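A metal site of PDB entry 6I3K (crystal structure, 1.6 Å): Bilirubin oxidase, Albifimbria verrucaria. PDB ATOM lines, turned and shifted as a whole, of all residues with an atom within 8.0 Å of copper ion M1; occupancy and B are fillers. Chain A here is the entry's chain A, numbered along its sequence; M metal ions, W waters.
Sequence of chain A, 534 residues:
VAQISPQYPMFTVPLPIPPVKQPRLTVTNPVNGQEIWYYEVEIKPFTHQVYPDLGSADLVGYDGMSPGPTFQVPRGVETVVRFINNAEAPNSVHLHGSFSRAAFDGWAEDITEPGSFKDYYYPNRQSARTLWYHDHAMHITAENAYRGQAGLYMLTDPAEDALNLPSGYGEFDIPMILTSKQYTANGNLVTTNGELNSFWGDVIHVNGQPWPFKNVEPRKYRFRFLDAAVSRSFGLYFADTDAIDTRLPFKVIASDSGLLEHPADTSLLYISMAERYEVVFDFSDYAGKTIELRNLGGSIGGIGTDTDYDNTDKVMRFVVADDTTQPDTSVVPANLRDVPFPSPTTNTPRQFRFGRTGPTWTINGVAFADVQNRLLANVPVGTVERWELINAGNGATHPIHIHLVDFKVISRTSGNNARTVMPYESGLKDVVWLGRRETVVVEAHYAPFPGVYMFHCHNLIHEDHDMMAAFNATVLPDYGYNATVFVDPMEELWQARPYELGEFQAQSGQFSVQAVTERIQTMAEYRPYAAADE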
ATOM      1  N   HIS A  94      25.925  18.626  15.857  1.00  0.00           N
ATOM      2  CA  HIS A  94      26.737  17.392  15.857  1.00  0.00           C
ATOM      3  C   HIS A  94      28.160  17.674  15.380  1.00  0.00           C
ATOM      4  O   HIS A  94      28.300  18.227  14.259  1.00  0.00           O
ATOM      5  CB  HIS A  94      26.128  16.330  14.947  1.00  0.00           C
ATOM      6  CG  HIS A  94      26.952  15.110  14.762  1.00  0.00           C
ATOM      7  ND1 HIS A  94      27.534  14.408  15.818  1.00  0.00           N
ATOM      8  CD2 HIS A  94      27.314  14.484  13.634  1.00  0.00           C
ATOM      9  CE1 HIS A  94      28.192  13.377  15.327  1.00  0.00           C
ATOM     10  NE2 HIS A  94      28.086  13.415  14.012  1.00  0.00           N
ATOM     11  N   LEU A  95      29.164  17.325  16.198  1.00  0.00           N
ATOM     12  CA  LEU A  95      30.581  17.350  15.746  1.00  0.00           C
ATOM     13  C   LEU A  95      30.871  15.995  15.120  1.00  0.00           C
ATOM     14  O   LEU A  95      31.124  14.993  15.827  1.00  0.00           O
ATOM     15  CB  LEU A  95      31.526  17.691  16.900  1.00  0.00           C
ATOM     16  CG  LEU A  95      33.012  17.728  16.550  1.00  0.00           C
ATOM     17  CD1 LEU A  95      33.308  18.765  15.486  1.00  0.00           C
ATOM     18  CD2 LEU A  95      33.837  18.053  17.796  1.00  0.00           C
ATOM     19  N   HIS A  96      30.799  15.977  13.797  1.00  0.00           N
ATOM     20  CA  HIS A  96      30.925  14.728  13.017  1.00  0.00           C
ATOM     21  C   HIS A  96      32.415  14.320  12.948  1.00  0.00           C
ATOM     22  O   HIS A  96      33.247  15.118  12.452  1.00  0.00           O
ATOM     23  CB  HIS A  96      30.292  14.956  11.637  1.00  0.00           C
ATOM     24  CG  HIS A  96      30.265  13.745  10.769  1.00  0.00           C
ATOM     25  ND1 HIS A  96      29.171  13.429   9.988  1.00  0.00           N
ATOM     26  CD2 HIS A  96      31.183  12.785  10.541  1.00  0.00           C
ATOM     27  CE1 HIS A  96      29.419  12.304   9.342  1.00  0.00           C
ATOM     28  NE2 HIS A  96      30.644  11.876   9.653  1.00  0.00           N
ATOM     29  N   GLY A  97      32.747  13.127  13.466  1.00  0.00           N
ATOM     30  CA  GLY A  97      34.127  12.605  13.514  1.00  0.00           C
ATOM     31  C   GLY A  97      34.676  12.562  14.931  1.00  0.00           C
ATOM     32  O   GLY A  97      35.839  12.144  15.118  1.00  0.00           O
ATOM     33  N   TRP A 132      33.785  17.951  10.994  1.00  0.00           N
ATOM     34  CA  TRP A 132      32.899  19.051  10.618  1.00  0.00           C
ATOM     35  C   TRP A 132      31.738  19.096  11.613  1.00  0.00           C
ATOM     36  O   TRP A 132      31.384  18.037  12.133  1.00  0.00           O
ATOM     37  CB  TRP A 132      32.455  18.982   9.149  1.00  0.00           C
ATOM     38  CG  TRP A 132      31.564  17.856   8.718  1.00  0.00           C
ATOM     39  CD1 TRP A 132      31.825  16.513   8.756  1.00  0.00           C
ATOM     40  CD2 TRP A 132      30.308  18.014   8.039  1.00  0.00           C
ATOM     41  NE1 TRP A 132      30.802  15.822   8.175  1.00  0.00           N
ATOM     42  CE2 TRP A 132      29.854  16.725   7.708  1.00  0.00           C
ATOM     43  CE3 TRP A 132      29.543  19.124   7.674  1.00  0.00           C
ATOM     44  CZ2 TRP A 132      28.637  16.541   7.026  1.00  0.00           C
ATOM     45  CZ3 TRP A 132      28.349  18.946   7.021  1.00  0.00           C
ATOM     46  CH2 TRP A 132      27.887  17.660   6.722  1.00  0.00           C
ATOM     47  N   TYR A 133      31.292  20.296  11.933  1.00  0.00           N
ATOM     48  CA  TYR A 133      30.131  20.491  12.844  1.00  0.00           C
ATOM     49  C   TYR A 133      28.945  20.954  12.013  1.00  0.00           C
ATOM     50  O   TYR A 133      29.101  21.792  11.109  1.00  0.00           O
ATOM     51  CB  TYR A 133      30.479  21.377  14.043  1.00  0.00           C
ATOM     52  CG  TYR A 133      30.808  22.812  13.708  1.00  0.00           C
ATOM     53  CD1 TYR A 133      32.043  23.196  13.146  1.00  0.00           C
ATOM     54  CD2 TYR A 133      29.884  23.834  13.927  1.00  0.00           C
ATOM     55  CE1 TYR A 133      32.343  24.502  12.809  1.00  0.00           C
ATOM     56  CE2 TYR A 133      30.175  25.153  13.618  1.00  0.00           C
ATOM     57  CZ  TYR A 133      31.402  25.518  13.066  1.00  0.00           C
ATOM     58  OH  TYR A 133      31.714  26.807  12.736  1.00  0.00           O
ATOM     59  N   HIS A 134      27.778  20.375  12.265  1.00  0.00           N
ATOM     60  CA  HIS A 134      26.584  20.712  11.451  1.00  0.00           C
ATOM     61  C   HIS A 134      25.308  20.481  12.252  1.00  0.00           C
ATOM     62  O   HIS A 134      25.294  19.743  13.256  1.00  0.00           O
ATOM     63  CB  HIS A 134      26.601  19.903  10.129  1.00  0.00           C
ATOM     64  CG  HIS A 134      26.460  18.434  10.293  1.00  0.00           C
ATOM     65  ND1 HIS A 134      25.230  17.806  10.461  1.00  0.00           N
ATOM     66  CD2 HIS A 134      27.365  17.425  10.201  1.00  0.00           C
ATOM     67  CE1 HIS A 134      25.420  16.496  10.541  1.00  0.00           C
ATOM     68  NE2 HIS A 134      26.710  16.237  10.300  1.00  0.00           N
ATOM     69  N   ASP A 135      24.214  21.036  11.728  1.00  0.00           N
ATOM     70  CA  ASP A 135      22.924  20.839  12.413  1.00  0.00           C
ATOM     71  C   ASP A 135      22.468  19.412  12.261  1.00  0.00           C
ATOM     72  O   ASP A 135      22.762  18.733  11.229  1.00  0.00           O
ATOM     73  CB  ASP A 135      21.827  21.775  11.893  1.00  0.00           C
ATOM     74  CG  ASP A 135      20.642  21.711  12.854  1.00  0.00           C
ATOM     75  OD1 ASP A 135      20.854  22.147  14.011  1.00  0.00           O
ATOM     76  OD2 ASP A 135      19.590  21.208  12.462  1.00  0.00           O
ATOM     77  N   HIS A 136      21.703  18.929  13.236  1.00  0.00           N
ATOM     78  CA  HIS A 136      21.169  17.564  13.280  1.00  0.00           C
ATOM     79  C   HIS A 136      19.745  17.518  13.854  1.00  0.00           C
ATOM     80  O   HIS A 136      19.333  16.404  14.250  1.00  0.00           O
ATOM     81  CB  HIS A 136      22.129  16.678  14.106  1.00  0.00           C
ATOM     82  CG  HIS A 136      22.308  15.307  13.571  1.00  0.00           C
ATOM     83  ND1 HIS A 136      21.244  14.422  13.343  1.00  0.00           N
ATOM     84  CD2 HIS A 136      23.443  14.632  13.228  1.00  0.00           C
ATOM     85  CE1 HIS A 136      21.736  13.289  12.822  1.00  0.00           C
ATOM     86  NE2 HIS A 136      23.093  13.360  12.739  1.00  0.00           N
ATOM     87  N   THR A 141      16.916  18.874   9.527  1.00  0.00           N
ATOM     88  CA  THR A 141      18.392  18.836   9.324  1.00  0.00           C
ATOM     89  C   THR A 141      18.722  19.317   7.906  1.00  0.00           C
ATOM     90  O   THR A 141      19.676  20.118   7.735  1.00  0.00           O
ATOM     91  CB  THR A 141      18.942  17.436   9.608  1.00  0.00           C
ATOM     92  OG1 THR A 141      18.822  17.184  11.004  1.00  0.00           O
ATOM     93  CG2 THR A 141      20.409  17.311   9.225  1.00  0.00           C
ATOM     94  N   LEU A 226      35.272  18.124   1.709  1.00  0.00           N
ATOM     95  CA  LEU A 226      34.102  17.723   2.521  1.00  0.00           C
ATOM     96  C   LEU A 226      32.878  17.826   1.600  1.00  0.00           C
ATOM     97  O   LEU A 226      32.669  18.910   1.007  1.00  0.00           O
ATOM     98  CB  LEU A 226      33.936  18.629   3.737  1.00  0.00           C
ATOM     99  CG  LEU A 226      32.574  18.569   4.426  1.00  0.00           C
ATOM    100  CD1 LEU A 226      32.283  17.205   5.014  1.00  0.00           C
ATOM    101  CD2 LEU A 226      32.440  19.642   5.492  1.00  0.00           C
ATOM    102  N   ASP A 227      32.093  16.756   1.491  1.00  0.00           N
ATOM    103  CA  ASP A 227      30.771  16.864   0.818  1.00  0.00           C
ATOM    104  C   ASP A 227      29.703  17.271   1.844  1.00  0.00           C
ATOM    105  O   ASP A 227      29.201  16.376   2.560  1.00  0.00           O
ATOM    106  CB  ASP A 227      30.426  15.597   0.059  1.00  0.00           C
ATOM    107  CG  ASP A 227      29.161  15.712  -0.754  1.00  0.00           C
ATOM    108  OD1 ASP A 227      28.476  16.761  -0.638  1.00  0.00           O
ATOM    109  OD2 ASP A 227      28.859  14.745  -1.527  1.00  0.00           O
ATOM    110  N   MET A 273      27.942  12.321   0.564  1.00  0.00           N
ATOM    111  CA  MET A 273      27.589  13.259   1.641  1.00  0.00           C
ATOM    112  C   MET A 273      28.244  12.831   2.971  1.00  0.00           C
ATOM    113  O   MET A 273      28.110  11.672   3.385  1.00  0.00           O
ATOM    114  CB  MET A 273      26.077  13.375   1.852  1.00  0.00           C
ATOM    115  CG  MET A 273      25.345  14.084   0.711  1.00  0.00           C
ATOM    116  SD  MET A 273      25.208  13.163  -0.849  1.00  0.00           S
ATOM    117  CE  MET A 273      23.944  11.951  -0.496  1.00  0.00           C
ATOM    118  N   ALA A 274      28.926  13.788   3.596  1.00  0.00           N
ATOM    119  CA  ALA A 274      29.549  13.744   4.942  1.00  0.00           C
ATOM    120  C   ALA A 274      30.950  13.127   4.902  1.00  0.00           C
ATOM    121  O   ALA A 274      31.648  13.153   5.933  1.00  0.00           O
ATOM    122  CB  ALA A 274      28.657  13.052   5.980  1.00  0.00           C
ATOM    123  N   GLU A 275      31.384  12.583   3.764  1.00  0.00           N
ATOM    124  CA  GLU A 275      32.766  12.060   3.624  1.00  0.00           C
ATOM    125  C   GLU A 275      33.761  13.231   3.583  1.00  0.00           C
ATOM    126  O   GLU A 275      33.454  14.302   3.012  1.00  0.00           O
ATOM    127  CB  GLU A 275      32.929  11.181   2.395  1.00  0.00           C
ATOM    128  CG  GLU A 275      32.167   9.858   2.520  1.00  0.00           C
ATOM    129  CD  GLU A 275      32.509   8.884   1.395  1.00  0.00           C
ATOM    130  OE1 GLU A 275      32.403   9.292   0.201  1.00  0.00           O
ATOM    131  OE2 GLU A 275      32.847   7.727   1.683  1.00  0.00           O
ATOM    132  N   ARG A 276      34.926  13.008   4.198  1.00  0.00           N
ATOM    133  CA  ARG A 276      36.109  13.904   4.092  1.00  0.00           C
ATOM    134  C   ARG A 276      37.237  13.109   3.451  1.00  0.00           C
ATOM    135  O   ARG A 276      37.536  12.008   3.914  1.00  0.00           O
ATOM    136  CB  ARG A 276      36.537  14.494   5.441  1.00  0.00           C
ATOM    137  CG  ARG A 276      35.537  15.452   6.085  1.00  0.00           C
ATOM    138  CD  ARG A 276      34.463  14.728   6.870  1.00  0.00           C
ATOM    139  NE  ARG A 276      35.003  14.069   8.052  1.00  0.00           N
ATOM    140  CZ  ARG A 276      34.475  12.981   8.629  1.00  0.00           C
ATOM    141  NH1 ARG A 276      35.013  12.512   9.742  1.00  0.00           N
ATOM    142  NH2 ARG A 276      33.388  12.401   8.110  1.00  0.00           N
ATOM    143  N   HIS A 401      26.359   6.550   7.762  1.00  0.00           N
ATOM    144  CA  HIS A 401      27.207   7.118   8.834  1.00  0.00           C
ATOM    145  C   HIS A 401      26.853   6.453  10.154  1.00  0.00           C
ATOM    146  O   HIS A 401      25.645   6.314  10.473  1.00  0.00           O
ATOM    147  CB  HIS A 401      27.013   8.640   8.918  1.00  0.00           C
ATOM    148  CG  HIS A 401      27.752   9.246  10.054  1.00  0.00           C
ATOM    149  ND1 HIS A 401      29.104   8.951  10.328  1.00  0.00           N
ATOM    150  CD2 HIS A 401      27.352  10.174  10.938  1.00  0.00           C
ATOM    151  CE1 HIS A 401      29.472   9.685  11.388  1.00  0.00           C
ATOM    152  NE2 HIS A 401      28.421  10.474  11.761  1.00  0.00           N
ATOM    153  N   HIS A 403      27.649   6.970  14.190  1.00  0.00           N
ATOM    154  CA  HIS A 403      28.243   7.849  15.213  1.00  0.00           C
ATOM    155  C   HIS A 403      29.165   7.034  16.128  1.00  0.00           C
ATOM    156  O   HIS A 403      29.176   5.793  16.073  1.00  0.00           O
ATOM    157  CB  HIS A 403      27.125   8.579  15.996  1.00  0.00           C
ATOM    158  CG  HIS A 403      26.447   9.712  15.281  1.00  0.00           C
ATOM    159  ND1 HIS A 403      26.257  10.919  15.874  1.00  0.00           N
ATOM    160  CD2 HIS A 403      25.853   9.792  14.071  1.00  0.00           C
ATOM    161  CE1 HIS A 403      25.616  11.733  15.044  1.00  0.00           C
ATOM    162  NE2 HIS A 403      25.365  11.069  13.911  1.00  0.00           N
ATOM    163  N   ASP A 430      34.168   6.921   8.715  1.00  0.00           N
ATOM    164  CA  ASP A 430      32.920   6.940   9.515  1.00  0.00           C
ATOM    165  C   ASP A 430      31.682   7.135   8.628  1.00  0.00           C
ATOM    166  O   ASP A 430      30.552   7.003   9.151  1.00  0.00           O
ATOM    167  CB  ASP A 430      32.989   7.966  10.661  1.00  0.00           C
ATOM    168  CG  ASP A 430      33.149   9.419  10.248  1.00  0.00           C
ATOM    169  OD1 ASP A 430      32.629   9.826   9.165  1.00  0.00           O
ATOM    170  OD2 ASP A 430      33.815  10.134  11.024  1.00  0.00           O
ATOM    171  N   VAL A 431      31.857   7.313   7.319  1.00  0.00           N
ATOM    172  CA  VAL A 431      30.759   7.258   6.313  1.00  0.00           C
ATOM    173  C   VAL A 431      31.203   6.297   5.209  1.00  0.00           C
ATOM    174  O   VAL A 431      32.398   6.319   4.859  1.00  0.00           O
ATOM    175  CB  VAL A 431      30.505   8.656   5.736  1.00  0.00           C
ATOM    176  CG1 VAL A 431      29.396   8.677   4.682  1.00  0.00           C
ATOM    177  CG2 VAL A 431      30.198   9.665   6.832  1.00  0.00           C
ATOM    178  N   HIS A 456      22.677   6.331  10.340  1.00  0.00           N
ATOM    179  CA  HIS A 456      21.714   6.847   9.349  1.00  0.00           C
ATOM    180  C   HIS A 456      22.362   6.972   7.987  1.00  0.00           C
ATOM    181  O   HIS A 456      23.593   7.052   7.862  1.00  0.00           O
ATOM    182  CB  HIS A 456      21.153   8.206   9.776  1.00  0.00           C
ATOM    183  CG  HIS A 456      22.174   9.279  10.037  1.00  0.00           C
ATOM    184  ND1 HIS A 456      22.439  10.257   9.138  1.00  0.00           N
ATOM    185  CD2 HIS A 456      22.926   9.565  11.128  1.00  0.00           C
ATOM    186  CE1 HIS A 456      23.260  11.146   9.676  1.00  0.00           C
ATOM    187  NE2 HIS A 456      23.620  10.719  10.878  1.00  0.00           N
ATOM    188  N   HIS A 458      23.246   9.683   5.269  1.00  0.00           N
ATOM    189  CA  HIS A 458      23.606  11.103   5.362  1.00  0.00           C
ATOM    190  C   HIS A 458      23.180  11.907   4.126  1.00  0.00           C
ATOM    191  O   HIS A 458      23.561  13.104   4.027  1.00  0.00           O
ATOM    192  CB  HIS A 458      25.110  11.232   5.711  1.00  0.00           C
ATOM    193  CG  HIS A 458      25.434  12.351   6.654  1.00  0.00           C
ATOM    194  ND1 HIS A 458      25.213  13.671   6.370  1.00  0.00           N
ATOM    195  CD2 HIS A 458      26.033  12.325   7.860  1.00  0.00           C
ATOM    196  CE1 HIS A 458      25.628  14.414   7.390  1.00  0.00           C
ATOM    197  NE2 HIS A 458      26.165  13.598   8.292  1.00  0.00           N
ATOM    198  N   LEU A 460      20.563  14.148   3.319  1.00  0.00           N
ATOM    199  CA  LEU A 460      19.823  14.815   4.425  1.00  0.00           C
ATOM    200  C   LEU A 460      18.306  14.701   4.158  1.00  0.00           C
ATOM    201  O   LEU A 460      17.532  14.681   5.142  1.00  0.00           O
ATOM    202  CB  LEU A 460      20.261  16.262   4.624  1.00  0.00           C
ATOM    203  CG  LEU A 460      21.779  16.449   4.855  1.00  0.00           C
ATOM    204  CD1 LEU A 460      22.066  17.923   5.082  1.00  0.00           C
ATOM    205  CD2 LEU A 460      22.320  15.651   6.027  1.00  0.00           C
ATOM    206  N   GLU A 463      17.507  11.168   5.413  1.00  0.00           N
ATOM    207  CA  GLU A 463      17.677  11.258   6.884  1.00  0.00           C
ATOM    208  C   GLU A 463      16.427  11.840   7.534  1.00  0.00           C
ATOM    209  O   GLU A 463      15.965  11.280   8.542  1.00  0.00           O
ATOM    210  CB  GLU A 463      18.916  12.134   7.141  1.00  0.00           C
ATOM    211  CG  GLU A 463      19.238  12.335   8.618  1.00  0.00           C
ATOM    212  CD  GLU A 463      20.557  13.062   8.842  1.00  0.00           C
ATOM    213  OE1 GLU A 463      21.450  12.978   7.958  1.00  0.00           O
ATOM    214  OE2 GLU A 463      20.668  13.751   9.904  1.00  0.00           O
HETATM  215 CU    CU M   1      27.452  14.433   9.779  1.00  0.00          CU
HETATM  216 CU    CU M   2      28.490  11.852  13.014  1.00  0.00          CU
HETATM  217 CU    CU M   3      24.232  11.782  12.467  1.00  0.00          CU
HETATM  218  O   HOH W   1      25.566  13.280  11.081  1.00  0.00           O
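His 94 touches copper ion M1 (CD2 to CU, 3.9 Å). CZ2 of Trp 132 touches copper ion M1 (3.7 Å). Five residues have an atom within 4 Å of copper ion M1: His 94, His 96, Trp 132, His 134 and His 458. The nearest printed residue that does not touch copper ion M1 is Ala 274 (4.2 Å).
A ring nitrogen (NE2) of His 96 lies within hydrogen-bond range of the guanidinium group (NH2) of Arg 276, 3.2 Å away. ND1 of His 401 sits close to NE2 of His 96, at 3.4 Å. O of Trp 132 is in hydrogen-bond range of N of His 96 (2.7 Å). The backbone carbonyl oxygen of His 134 sits at hydrogen-bond distance from the backbone NH of His 94 (2.9 Å). The side-chain carboxylate (OD1) of Asp 430 lies within hydrogen-bond range of a ring nitrogen (NE2) of His 96 (2.9 Å).
Copper ion M1 is bound by ND1 of His 96 (2.0 Å), NE2 of His 134 (2.0 Å), NE2 of His 458 (2.1 Å) and water W1 (2.6 Å).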
